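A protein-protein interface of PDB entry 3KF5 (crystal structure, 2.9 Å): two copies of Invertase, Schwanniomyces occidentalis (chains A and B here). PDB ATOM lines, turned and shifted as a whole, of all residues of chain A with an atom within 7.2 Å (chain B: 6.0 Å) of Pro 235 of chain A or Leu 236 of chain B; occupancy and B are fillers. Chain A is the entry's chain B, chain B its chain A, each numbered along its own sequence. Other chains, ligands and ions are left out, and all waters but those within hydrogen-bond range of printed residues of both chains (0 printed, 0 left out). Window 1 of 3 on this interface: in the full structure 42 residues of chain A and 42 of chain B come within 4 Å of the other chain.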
ATOM      1  N   TYR A 201     -12.520 -19.201 -10.126  1.00  0.00           N
ATOM      2  CA  TYR A 201     -13.595 -19.719 -10.956  1.00  0.00           C
ATOM      3  C   TYR A 201     -13.681 -18.916 -12.242  1.00  0.00           C
ATOM      4  O   TYR A 201     -13.981 -17.719 -12.214  1.00  0.00           O
ATOM      5  CB  TYR A 201     -14.924 -19.651 -10.206  1.00  0.00           C
ATOM      6  CG  TYR A 201     -15.872 -20.754 -10.590  1.00  0.00           C
ATOM      7  CD1 TYR A 201     -15.775 -22.025  -9.991  1.00  0.00           C
ATOM      8  CD2 TYR A 201     -16.853 -20.552 -11.566  1.00  0.00           C
ATOM      9  CE1 TYR A 201     -16.638 -23.059 -10.349  1.00  0.00           C
ATOM     10  CE2 TYR A 201     -17.723 -21.584 -11.935  1.00  0.00           C
ATOM     11  CZ  TYR A 201     -17.610 -22.828 -11.319  1.00  0.00           C
ATOM     12  OH  TYR A 201     -18.469 -23.844 -11.671  1.00  0.00           O
ATOM     13  N   GLY A 203     -15.680 -19.371 -15.187  1.00  0.00           N
ATOM     14  CA  GLY A 203     -16.979 -19.133 -15.810  1.00  0.00           C
ATOM     15  C   GLY A 203     -16.837 -18.724 -17.271  1.00  0.00           C
ATOM     16  O   GLY A 203     -15.970 -19.242 -17.990  1.00  0.00           O
ATOM     17  N   ILE A 230     -17.290 -12.454 -12.225  1.00  0.00           N
ATOM     18  CA  ILE A 230     -17.520 -13.301 -13.388  1.00  0.00           C
ATOM     19  C   ILE A 230     -19.010 -13.394 -13.708  1.00  0.00           C
ATOM     20  O   ILE A 230     -19.849 -13.413 -12.804  1.00  0.00           O
ATOM     21  CB  ILE A 230     -16.917 -14.717 -13.212  1.00  0.00           C
ATOM     22  CG1 ILE A 230     -17.496 -15.408 -11.972  1.00  0.00           C
ATOM     23  CG2 ILE A 230     -15.384 -14.649 -13.161  1.00  0.00           C
ATOM     24  CD1 ILE A 230     -17.430 -16.912 -12.009  1.00  0.00           C
ATOM     25  N   PRO A 232     -21.395 -15.000 -17.463  1.00  0.00           N
ATOM     26  CA  PRO A 232     -22.381 -15.835 -16.780  1.00  0.00           C
ATOM     27  C   PRO A 232     -21.924 -17.228 -16.305  1.00  0.00           C
ATOM     28  O   PRO A 232     -22.692 -18.199 -16.378  1.00  0.00           O
ATOM     29  CB  PRO A 232     -23.484 -15.971 -17.837  1.00  0.00           C
ATOM     30  CG  PRO A 232     -22.755 -15.939 -19.105  1.00  0.00           C
ATOM     31  CD  PRO A 232     -21.688 -14.914 -18.904  1.00  0.00           C
ATOM     32  N   GLY A 233     -20.716 -17.343 -15.783  1.00  0.00           N
ATOM     33  CA  GLY A 233     -20.282 -18.656 -15.307  1.00  0.00           C
ATOM     34  C   GLY A 233     -20.638 -19.095 -13.889  1.00  0.00           C
ATOM     35  O   GLY A 233     -20.377 -20.243 -13.522  1.00  0.00           O
ATOM     36  N   SER A 234     -21.226 -18.204 -13.091  1.00  0.00           N
ATOM     37  CA  SER A 234     -21.372 -18.439 -11.644  1.00  0.00           C
ATOM     38  C   SER A 234     -21.887 -19.840 -11.311  1.00  0.00           C
ATOM     39  O   SER A 234     -22.927 -20.259 -11.827  1.00  0.00           O
ATOM     40  CB  SER A 234     -22.273 -17.381 -11.000  1.00  0.00           C
ATOM     41  OG  SER A 234     -22.509 -17.664  -9.630  1.00  0.00           O
ATOM     42  N   PRO A 235     -21.171 -20.566 -10.436  1.00  0.00           N
ATOM     43  CA  PRO A 235     -21.644 -21.899 -10.058  1.00  0.00           C
ATOM     44  C   PRO A 235     -23.047 -21.849  -9.425  1.00  0.00           C
ATOM     45  O   PRO A 235     -23.789 -22.819  -9.509  1.00  0.00           O
ATOM     46  CB  PRO A 235     -20.597 -22.371  -9.042  1.00  0.00           C
ATOM     47  CG  PRO A 235     -19.998 -21.127  -8.502  1.00  0.00           C
ATOM     48  CD  PRO A 235     -20.015 -20.137  -9.632  1.00  0.00           C
ATOM     49  N   LEU A 236     -23.390 -20.710  -8.823  1.00  0.00           N
ATOM     50  CA  LEU A 236     -24.691 -20.483  -8.198  1.00  0.00           C
ATOM     51  C   LEU A 236     -25.802 -20.112  -9.167  1.00  0.00           C
ATOM     52  O   LEU A 236     -26.984 -20.198  -8.807  1.00  0.00           O
ATOM     53  CB  LEU A 236     -24.591 -19.352  -7.175  1.00  0.00           C
ATOM     54  CG  LEU A 236     -24.475 -19.661  -5.687  1.00  0.00           C
ATOM     55  CD1 LEU A 236     -23.105 -20.228  -5.354  1.00  0.00           C
ATOM     56  CD2 LEU A 236     -24.731 -18.375  -4.924  1.00  0.00           C
ATOM     57  N   GLY A 237     -25.428 -19.669 -10.371  1.00  0.00           N
ATOM     58  CA  GLY A 237     -26.391 -19.104 -11.314  1.00  0.00           C
ATOM     59  C   GLY A 237     -25.760 -18.229 -12.378  1.00  0.00           C
ATOM     60  O   GLY A 237     -25.040 -18.721 -13.242  1.00  0.00           O
ATOM     61  N   GLY A 238     -26.020 -16.932 -12.346  1.00  0.00           N
ATOM     62  CA  GLY A 238     -25.549 -16.097 -13.446  1.00  0.00           C
ATOM     63  C   GLY A 238     -24.226 -15.414 -13.171  1.00  0.00           C
ATOM     64  O   GLY A 238     -23.160 -15.895 -13.573  1.00  0.00           O
ATOM     65  N   SER A 239     -24.326 -14.281 -12.479  1.00  0.00           N
ATOM     66  CA  SER A 239     -23.202 -13.449 -12.091  1.00  0.00           C
ATOM     67  C   SER A 239     -22.815 -13.703 -10.622  1.00  0.00           C
ATOM     68  O   SER A 239     -23.645 -14.170  -9.826  1.00  0.00           O
ATOM     69  CB  SER A 239     -23.582 -11.983 -12.305  1.00  0.00           C
ATOM     70  OG  SER A 239     -24.889 -11.699 -11.809  1.00  0.00           O
ATOM     71  N   ILE A 240     -21.554 -13.407 -10.282  1.00  0.00           N
ATOM     72  CA  ILE A 240     -21.022 -13.530  -8.911  1.00  0.00           C
ATOM     73  C   ILE A 240     -19.654 -12.835  -8.773  1.00  0.00           C
ATOM     74  O   ILE A 240     -18.982 -12.585  -9.776  1.00  0.00           O
ATOM     75  CB  ILE A 240     -20.932 -15.010  -8.459  1.00  0.00           C
ATOM     76  CG1 ILE A 240     -20.952 -15.116  -6.930  1.00  0.00           C
ATOM     77  CG2 ILE A 240     -19.717 -15.703  -9.080  1.00  0.00           C
ATOM     78  CD1 ILE A 240     -21.168 -16.540  -6.385  1.00  0.00           C
ATOM     79  N   THR A 260     -10.477 -20.976  -4.295  1.00  0.00           N
ATOM     80  CA  THR A 260     -11.526 -20.099  -4.790  1.00  0.00           C
ATOM     81  C   THR A 260     -12.480 -19.751  -3.642  1.00  0.00           C
ATOM     82  O   THR A 260     -12.917 -20.630  -2.903  1.00  0.00           O
ATOM     83  CB  THR A 260     -12.277 -20.771  -5.963  1.00  0.00           C
ATOM     84  OG1 THR A 260     -11.320 -21.161  -6.948  1.00  0.00           O
ATOM     85  CG2 THR A 260     -13.256 -19.829  -6.615  1.00  0.00           C
ATOM     86  N   PHE A 262     -15.865 -16.887  -2.748  1.00  0.00           N
ATOM     87  CA  PHE A 262     -16.745 -15.828  -3.232  1.00  0.00           C
ATOM     88  C   PHE A 262     -16.959 -14.740  -2.180  1.00  0.00           C
ATOM     89  O   PHE A 262     -16.953 -15.009  -0.980  1.00  0.00           O
ATOM     90  CB  PHE A 262     -18.066 -16.412  -3.738  1.00  0.00           C
ATOM     91  CG  PHE A 262     -17.893 -17.385  -4.872  1.00  0.00           C
ATOM     92  CD1 PHE A 262     -18.102 -18.752  -4.678  1.00  0.00           C
ATOM     93  CD2 PHE A 262     -17.492 -16.940  -6.132  1.00  0.00           C
ATOM     94  CE1 PHE A 262     -17.933 -19.657  -5.723  1.00  0.00           C
ATOM     95  CE2 PHE A 262     -17.321 -17.832  -7.181  1.00  0.00           C
ATOM     96  CZ  PHE A 262     -17.537 -19.195  -6.975  1.00  0.00           C
ATOM     97  N   LYS A 435     -33.971 -20.999  -2.805  1.00  0.00           N
ATOM     98  CA  LYS A 435     -33.375 -21.627  -1.612  1.00  0.00           C
ATOM     99  C   LYS A 435     -31.852 -21.634  -1.633  1.00  0.00           C
ATOM    100  O   LYS A 435     -31.244 -22.208  -2.539  1.00  0.00           O
ATOM    101  CB  LYS A 435     -33.876 -23.059  -1.455  1.00  0.00           C
ATOM    102  CG  LYS A 435     -35.371 -23.175  -1.263  1.00  0.00           C
ATOM    103  CD  LYS A 435     -35.768 -24.611  -1.107  1.00  0.00           C
ATOM    104  CE  LYS A 435     -37.256 -24.743  -0.909  1.00  0.00           C
ATOM    105  NZ  LYS A 435     -37.563 -26.082  -0.328  1.00  0.00           N
ATOM    106  N   LEU A 436     -31.234 -21.023  -0.623  1.00  0.00           N
ATOM    107  CA  LEU A 436     -29.785 -20.832  -0.654  1.00  0.00           C
ATOM    108  C   LEU A 436     -28.966 -21.134   0.607  1.00  0.00           C
ATOM    109  O   LEU A 436     -29.325 -20.740   1.712  1.00  0.00           O
ATOM    110  CB  LEU A 436     -29.440 -19.421  -1.155  1.00  0.00           C
ATOM    111  CG  LEU A 436     -29.721 -19.095  -2.623  1.00  0.00           C
ATOM    112  CD1 LEU A 436     -29.626 -17.602  -2.854  1.00  0.00           C
ATOM    113  CD2 LEU A 436     -28.788 -19.857  -3.563  1.00  0.00           C
ATOM    114  N   ALA A 437     -27.910 -21.922   0.383  1.00  0.00           N
ATOM    115  CA  ALA A 437     -26.540 -21.756   0.946  1.00  0.00           C
ATOM    116  C   ALA A 437     -26.283 -21.653   2.435  1.00  0.00           C
ATOM    117  O   ALA A 437     -27.145 -21.949   3.247  1.00  0.00           O
ATOM    118  CB  ALA A 437     -25.791 -20.586   0.208  1.00  0.00           C
ATOM    119  N   GLY B 233     -18.885 -27.878   2.390  1.00  0.00           N
ATOM    120  CA  GLY B 233     -18.661 -26.534   1.859  1.00  0.00           C
ATOM    121  C   GLY B 233     -19.244 -26.148   0.500  1.00  0.00           C
ATOM    122  O   GLY B 233     -19.131 -24.986   0.100  1.00  0.00           O
ATOM    123  N   SER B 234     -19.857 -27.096  -0.215  1.00  0.00           N
ATOM    124  CA  SER B 234     -20.251 -26.876  -1.622  1.00  0.00           C
ATOM    125  C   SER B 234     -20.932 -25.533  -1.873  1.00  0.00           C
ATOM    126  O   SER B 234     -21.918 -25.199  -1.210  1.00  0.00           O
ATOM    127  CB  SER B 234     -21.155 -27.997  -2.138  1.00  0.00           C
ATOM    128  OG  SER B 234     -21.622 -27.723  -3.458  1.00  0.00           O
ATOM    129  N   PRO B 235     -20.426 -24.764  -2.853  1.00  0.00           N
ATOM    130  CA  PRO B 235     -21.054 -23.477  -3.141  1.00  0.00           C
ATOM    131  C   PRO B 235     -22.522 -23.656  -3.531  1.00  0.00           C
ATOM    132  O   PRO B 235     -23.333 -22.748  -3.317  1.00  0.00           O
ATOM    133  CB  PRO B 235     -20.225 -22.929  -4.311  1.00  0.00           C
ATOM    134  CG  PRO B 235     -19.581 -24.095  -4.921  1.00  0.00           C
ATOM    135  CD  PRO B 235     -19.366 -25.094  -3.821  1.00  0.00           C
ATOM    136  N   LEU B 236     -22.849 -24.833  -4.063  1.00  0.00           N
ATOM    137  CA  LEU B 236     -24.211 -25.181  -4.478  1.00  0.00           C
ATOM    138  C   LEU B 236     -25.139 -25.643  -3.352  1.00  0.00           C
ATOM    139  O   LEU B 236     -26.367 -25.677  -3.530  1.00  0.00           O
ATOM    140  CB  LEU B 236     -24.174 -26.293  -5.525  1.00  0.00           C
ATOM    141  CG  LEU B 236     -24.352 -25.946  -6.988  1.00  0.00           C
ATOM    142  CD1 LEU B 236     -23.096 -25.255  -7.508  1.00  0.00           C
ATOM    143  CD2 LEU B 236     -24.617 -27.244  -7.732  1.00  0.00           C
ATOM    144  N   GLY B 237     -24.564 -26.029  -2.215  1.00  0.00           N
ATOM    145  CA  GLY B 237     -25.331 -26.682  -1.168  1.00  0.00           C
ATOM    146  C   GLY B 237     -24.455 -27.467  -0.220  1.00  0.00           C
ATOM    147  O   GLY B 237     -23.648 -26.899   0.514  1.00  0.00           O
ATOM    148  N   GLY B 238     -24.601 -28.780  -0.211  1.00  0.00           N
ATOM    149  CA  GLY B 238     -23.914 -29.565   0.808  1.00  0.00           C
ATOM    150  C   GLY B 238     -22.613 -30.129   0.297  1.00  0.00           C
ATOM    151  O   GLY B 238     -21.540 -29.558   0.513  1.00  0.00           O
ATOM    152  N   SER B 239     -22.733 -31.252  -0.400  1.00  0.00           N
ATOM    153  CA  SER B 239     -21.597 -31.990  -0.931  1.00  0.00           C
ATOM    154  C   SER B 239     -21.440 -31.739  -2.432  1.00  0.00           C
ATOM    155  O   SER B 239     -22.412 -31.380  -3.106  1.00  0.00           O
ATOM    156  CB  SER B 239     -21.789 -33.479  -0.646  1.00  0.00           C
ATOM    157  OG  SER B 239     -23.115 -33.893  -0.941  1.00  0.00           O
ATOM    158  N   ILE B 240     -20.212 -31.908  -2.935  1.00  0.00           N
ATOM    159  CA  ILE B 240     -19.894 -31.763  -4.373  1.00  0.00           C
ATOM    160  C   ILE B 240     -18.528 -32.387  -4.732  1.00  0.00           C
ATOM    161  O   ILE B 240     -17.692 -32.615  -3.846  1.00  0.00           O
ATOM    162  CB  ILE B 240     -19.966 -30.269  -4.845  1.00  0.00           C
ATOM    163  CG1 ILE B 240     -20.184 -30.173  -6.363  1.00  0.00           C
ATOM    164  CG2 ILE B 240     -18.748 -29.490  -4.381  1.00  0.00           C
ATOM    165  CD1 ILE B 240     -20.716 -28.818  -6.831  1.00  0.00           C
ATOM    166  N   PHE B 262     -16.032 -28.028 -11.235  1.00  0.00           N
ATOM    167  CA  PHE B 262     -16.746 -29.141 -10.622  1.00  0.00           C
ATOM    168  C   PHE B 262     -17.033 -30.257 -11.621  1.00  0.00           C
ATOM    169  O   PHE B 262     -17.254 -30.004 -12.806  1.00  0.00           O
ATOM    170  CB  PHE B 262     -18.021 -28.647  -9.940  1.00  0.00           C
ATOM    171  CG  PHE B 262     -17.762 -27.667  -8.833  1.00  0.00           C
ATOM    172  CD1 PHE B 262     -18.113 -26.331  -8.976  1.00  0.00           C
ATOM    173  CD2 PHE B 262     -17.135 -28.075  -7.654  1.00  0.00           C
ATOM    174  CE1 PHE B 262     -17.867 -25.415  -7.958  1.00  0.00           C
ATOM    175  CE2 PHE B 262     -16.876 -27.168  -6.638  1.00  0.00           C
ATOM    176  CZ  PHE B 262     -17.245 -25.834  -6.788  1.00  0.00           C
ATOM    177  N   ASP B 264     -19.579 -32.360 -11.584  1.00  0.00           N
ATOM    178  CA  ASP B 264     -20.996 -32.423 -11.879  1.00  0.00           C
ATOM    179  C   ASP B 264     -21.647 -31.263 -11.143  1.00  0.00           C
ATOM    180  O   ASP B 264     -21.415 -31.099  -9.948  1.00  0.00           O
ATOM    181  CB  ASP B 264     -21.536 -33.766 -11.395  1.00  0.00           C
ATOM    182  CG  ASP B 264     -22.984 -33.984 -11.751  1.00  0.00           C
ATOM    183  OD1 ASP B 264     -23.840 -33.256 -11.200  1.00  0.00           O
ATOM    184  OD2 ASP B 264     -23.273 -34.901 -12.560  1.00  0.00           O
ATOM    185  N   ILE B 265     -22.432 -30.441 -11.844  1.00  0.00           N
ATOM    186  CA  ILE B 265     -23.106 -29.314 -11.183  1.00  0.00           C
ATOM    187  C   ILE B 265     -24.582 -29.539 -10.858  1.00  0.00           C
ATOM    188  O   ILE B 265     -25.382 -28.594 -10.796  1.00  0.00           O
ATOM    189  CB  ILE B 265     -22.916 -27.966 -11.902  1.00  0.00           C
ATOM    190  CG1 ILE B 265     -23.068 -28.123 -13.416  1.00  0.00           C
ATOM    191  CG2 ILE B 265     -21.594 -27.333 -11.479  1.00  0.00           C
ATOM    192  CD1 ILE B 265     -23.069 -26.792 -14.168  1.00  0.00           C
ATOM    193  N   GLY B 266     -24.928 -30.803 -10.647  1.00  0.00           N
ATOM    194  CA  GLY B 266     -26.171 -31.146  -9.980  1.00  0.00           C
ATOM    195  C   GLY B 266     -25.929 -31.115  -8.479  1.00  0.00           C
ATOM    196  O   GLY B 266     -24.804 -30.918  -8.018  1.00  0.00           O
ATOM    197  N   LYS B 267     -26.988 -31.322  -7.711  1.00  0.00           N
ATOM    198  CA  LYS B 267     -26.906 -31.320  -6.259  1.00  0.00           C
ATOM    199  C   LYS B 267     -26.442 -32.695  -5.714  1.00  0.00           C
ATOM    200  O   LYS B 267     -25.971 -32.796  -4.582  1.00  0.00           O
ATOM    201  CB  LYS B 267     -28.285 -30.947  -5.706  1.00  0.00           C
ATOM    202  CG  LYS B 267     -28.281 -30.205  -4.395  1.00  0.00           C
ATOM    203  CD  LYS B 267     -28.135 -28.701  -4.578  1.00  0.00           C
ATOM    204  CE  LYS B 267     -28.512 -27.941  -3.292  1.00  0.00           C
ATOM    205  NZ  LYS B 267     -27.917 -28.455  -2.026  1.00  0.00           N
ATOM    206  N   GLN B 292     -26.727 -33.152   2.883  1.00  0.00           N
ATOM    207  CA  GLN B 292     -27.624 -32.348   3.723  1.00  0.00           C
ATOM    208  C   GLN B 292     -29.061 -32.851   3.836  1.00  0.00           C
ATOM    209  O   GLN B 292     -29.798 -32.413   4.713  1.00  0.00           O
ATOM    210  CB  GLN B 292     -27.588 -30.849   3.374  1.00  0.00           C
ATOM    211  CG  GLN B 292     -27.515 -30.483   1.905  1.00  0.00           C
ATOM    212  CD  GLN B 292     -27.300 -28.994   1.688  1.00  0.00           C
ATOM    213  OE1 GLN B 292     -27.784 -28.424   0.713  1.00  0.00           O
ATOM    214  NE2 GLN B 292     -26.579 -28.357   2.596  1.00  0.00           N
ATOM    215  N   PHE B 431     -32.718 -27.188   1.916  1.00  0.00           N
ATOM    216  CA  PHE B 431     -31.450 -27.478   1.292  1.00  0.00           C
ATOM    217  C   PHE B 431     -31.682 -28.185  -0.047  1.00  0.00           C
ATOM    218  O   PHE B 431     -30.784 -28.254  -0.887  1.00  0.00           O
ATOM    219  CB  PHE B 431     -30.600 -28.314   2.246  1.00  0.00           C
ATOM    220  CG  PHE B 431     -30.380 -27.667   3.594  1.00  0.00           C
ATOM    221  CD1 PHE B 431     -30.898 -28.237   4.752  1.00  0.00           C
ATOM    222  CD2 PHE B 431     -29.663 -26.480   3.705  1.00  0.00           C
ATOM    223  CE1 PHE B 431     -30.702 -27.639   6.008  1.00  0.00           C
ATOM    224  CE2 PHE B 431     -29.463 -25.871   4.956  1.00  0.00           C
ATOM    225  CZ  PHE B 431     -29.984 -26.455   6.109  1.00  0.00           C
ATOM    226  N   THR B 433     -32.732 -28.104  -3.488  1.00  0.00           N
ATOM    227  CA  THR B 433     -32.697 -26.825  -4.216  1.00  0.00           C
ATOM    228  C   THR B 433     -33.746 -26.488  -5.304  1.00  0.00           C
ATOM    229  O   THR B 433     -34.146 -25.304  -5.429  1.00  0.00           O
ATOM    230  CB  THR B 433     -31.262 -26.431  -4.622  1.00  0.00           C
ATOM    231  OG1 THR B 433     -30.580 -25.950  -3.462  1.00  0.00           O
ATOM    232  CG2 THR B 433     -31.250 -25.315  -5.673  1.00  0.00           C
ATOM    233  N   LEU B 436     -31.842 -25.240 -11.012  1.00  0.00           N
ATOM    234  CA  LEU B 436     -30.388 -25.308 -11.200  1.00  0.00           C
ATOM    235  C   LEU B 436     -29.782 -24.935 -12.561  1.00  0.00           C
ATOM    236  O   LEU B 436     -30.254 -25.354 -13.616  1.00  0.00           O
ATOM    237  CB  LEU B 436     -29.837 -26.665 -10.744  1.00  0.00           C
ATOM    238  CG  LEU B 436     -29.879 -26.986  -9.242  1.00  0.00           C
ATOM    239  CD1 LEU B 436     -29.674 -28.474  -8.993  1.00  0.00           C
ATOM    240  CD2 LEU B 436     -28.871 -26.168  -8.451  1.00  0.00           C
ATOM    241  N   ALA B 437     -28.780 -24.056 -12.468  1.00  0.00           N
ATOM    242  CA  ALA B 437     -27.511 -24.071 -13.232  1.00  0.00           C
ATOM    243  C   ALA B 437     -27.487 -24.150 -14.753  1.00  0.00           C
ATOM    244  O   ALA B 437     -28.503 -23.962 -15.415  1.00  0.00           O
ATOM    245  CB  ALA B 437     -26.539 -25.150 -12.631  1.00  0.00           C
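Pro 235 of chain A touches Leu 236 of chain B, and with the chains exchanged Leu 236 of chain A touches Pro 235 of chain B.
Positions printed for both chains: 233, 234, 235, 236, 237, 238, 239, 240, 262, 436 and 437.
Among the printed residues, merely in contact across the chains: Tyr 201 of chain A with Phe 262 of chain B (3.6 Å), Pro 235 of chain A with Leu 236 of chain B (3.2 Å), Leu 236 of chain A with Pro 235 of chain B (3.2 Å) and Lys 435 of chain A with Thr 433 of chain B (3.9 Å).
Of the printed residues of chain B, Tyr 201 of chain A touches Phe 262 (3.6 Å).
Pro 235 of chain A touches just one residue of chain B: Leu 236 (3.2 Å).
Ile 240 of chain A touches none of the printed residues of chain B.
Of the printed residues of chain A, Leu 236 of chain B touches Pro 235 (3.2 Å).
Of the printed residues of chain A, Thr 433 of chain B touches Lys 435 (3.9 Å).
The nearest residue of chain B that does not touch Pro 235 of chain A is Phe 262 of chain B (4.2 Å).
The nearest residue of chain A that does not touch Leu 236 of chain B is Leu 236 of chain A (4.7 Å).
The nearest printed residue of chain A that does not touch Phe 262 of chain B is Pro 235 of chain A (4.2 Å).
OG of Ser 234 of chain B lies close to N of Leu 236 of chain B (3.2 Å).
O of Phe 431 of chain B lies within hydrogen-bond range of OG1 of Thr 433 of chain B (3.5 Å).
The backbone NH (N) of Leu 236 of chain A lies close to the side-chain hydroxyl (OG) of Ser 234 of chain A (3.3 Å).
Of the 17 printed residues of chain A, 4 touch a printed residue of chain B.
Printed residues of chain A that touch a printed residue of chain B: Tyr 201, Pro 235, Leu 236 and Lys 435.
Hydrophobic or aromatic side chains of chain A that line the printed part of chain B: Tyr 201 and Leu 236.
Hydrophobic or aromatic side chains of chain B within 4 Å of the printed part of chain A: Leu 236 and Phe 262.
Among the printed residues, 4 pairs touch across the chains.
Among the printed residues, no Asp or Glu carboxylate lies within 4 Å of a Lys or Arg side-chain nitrogen of the other chain.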
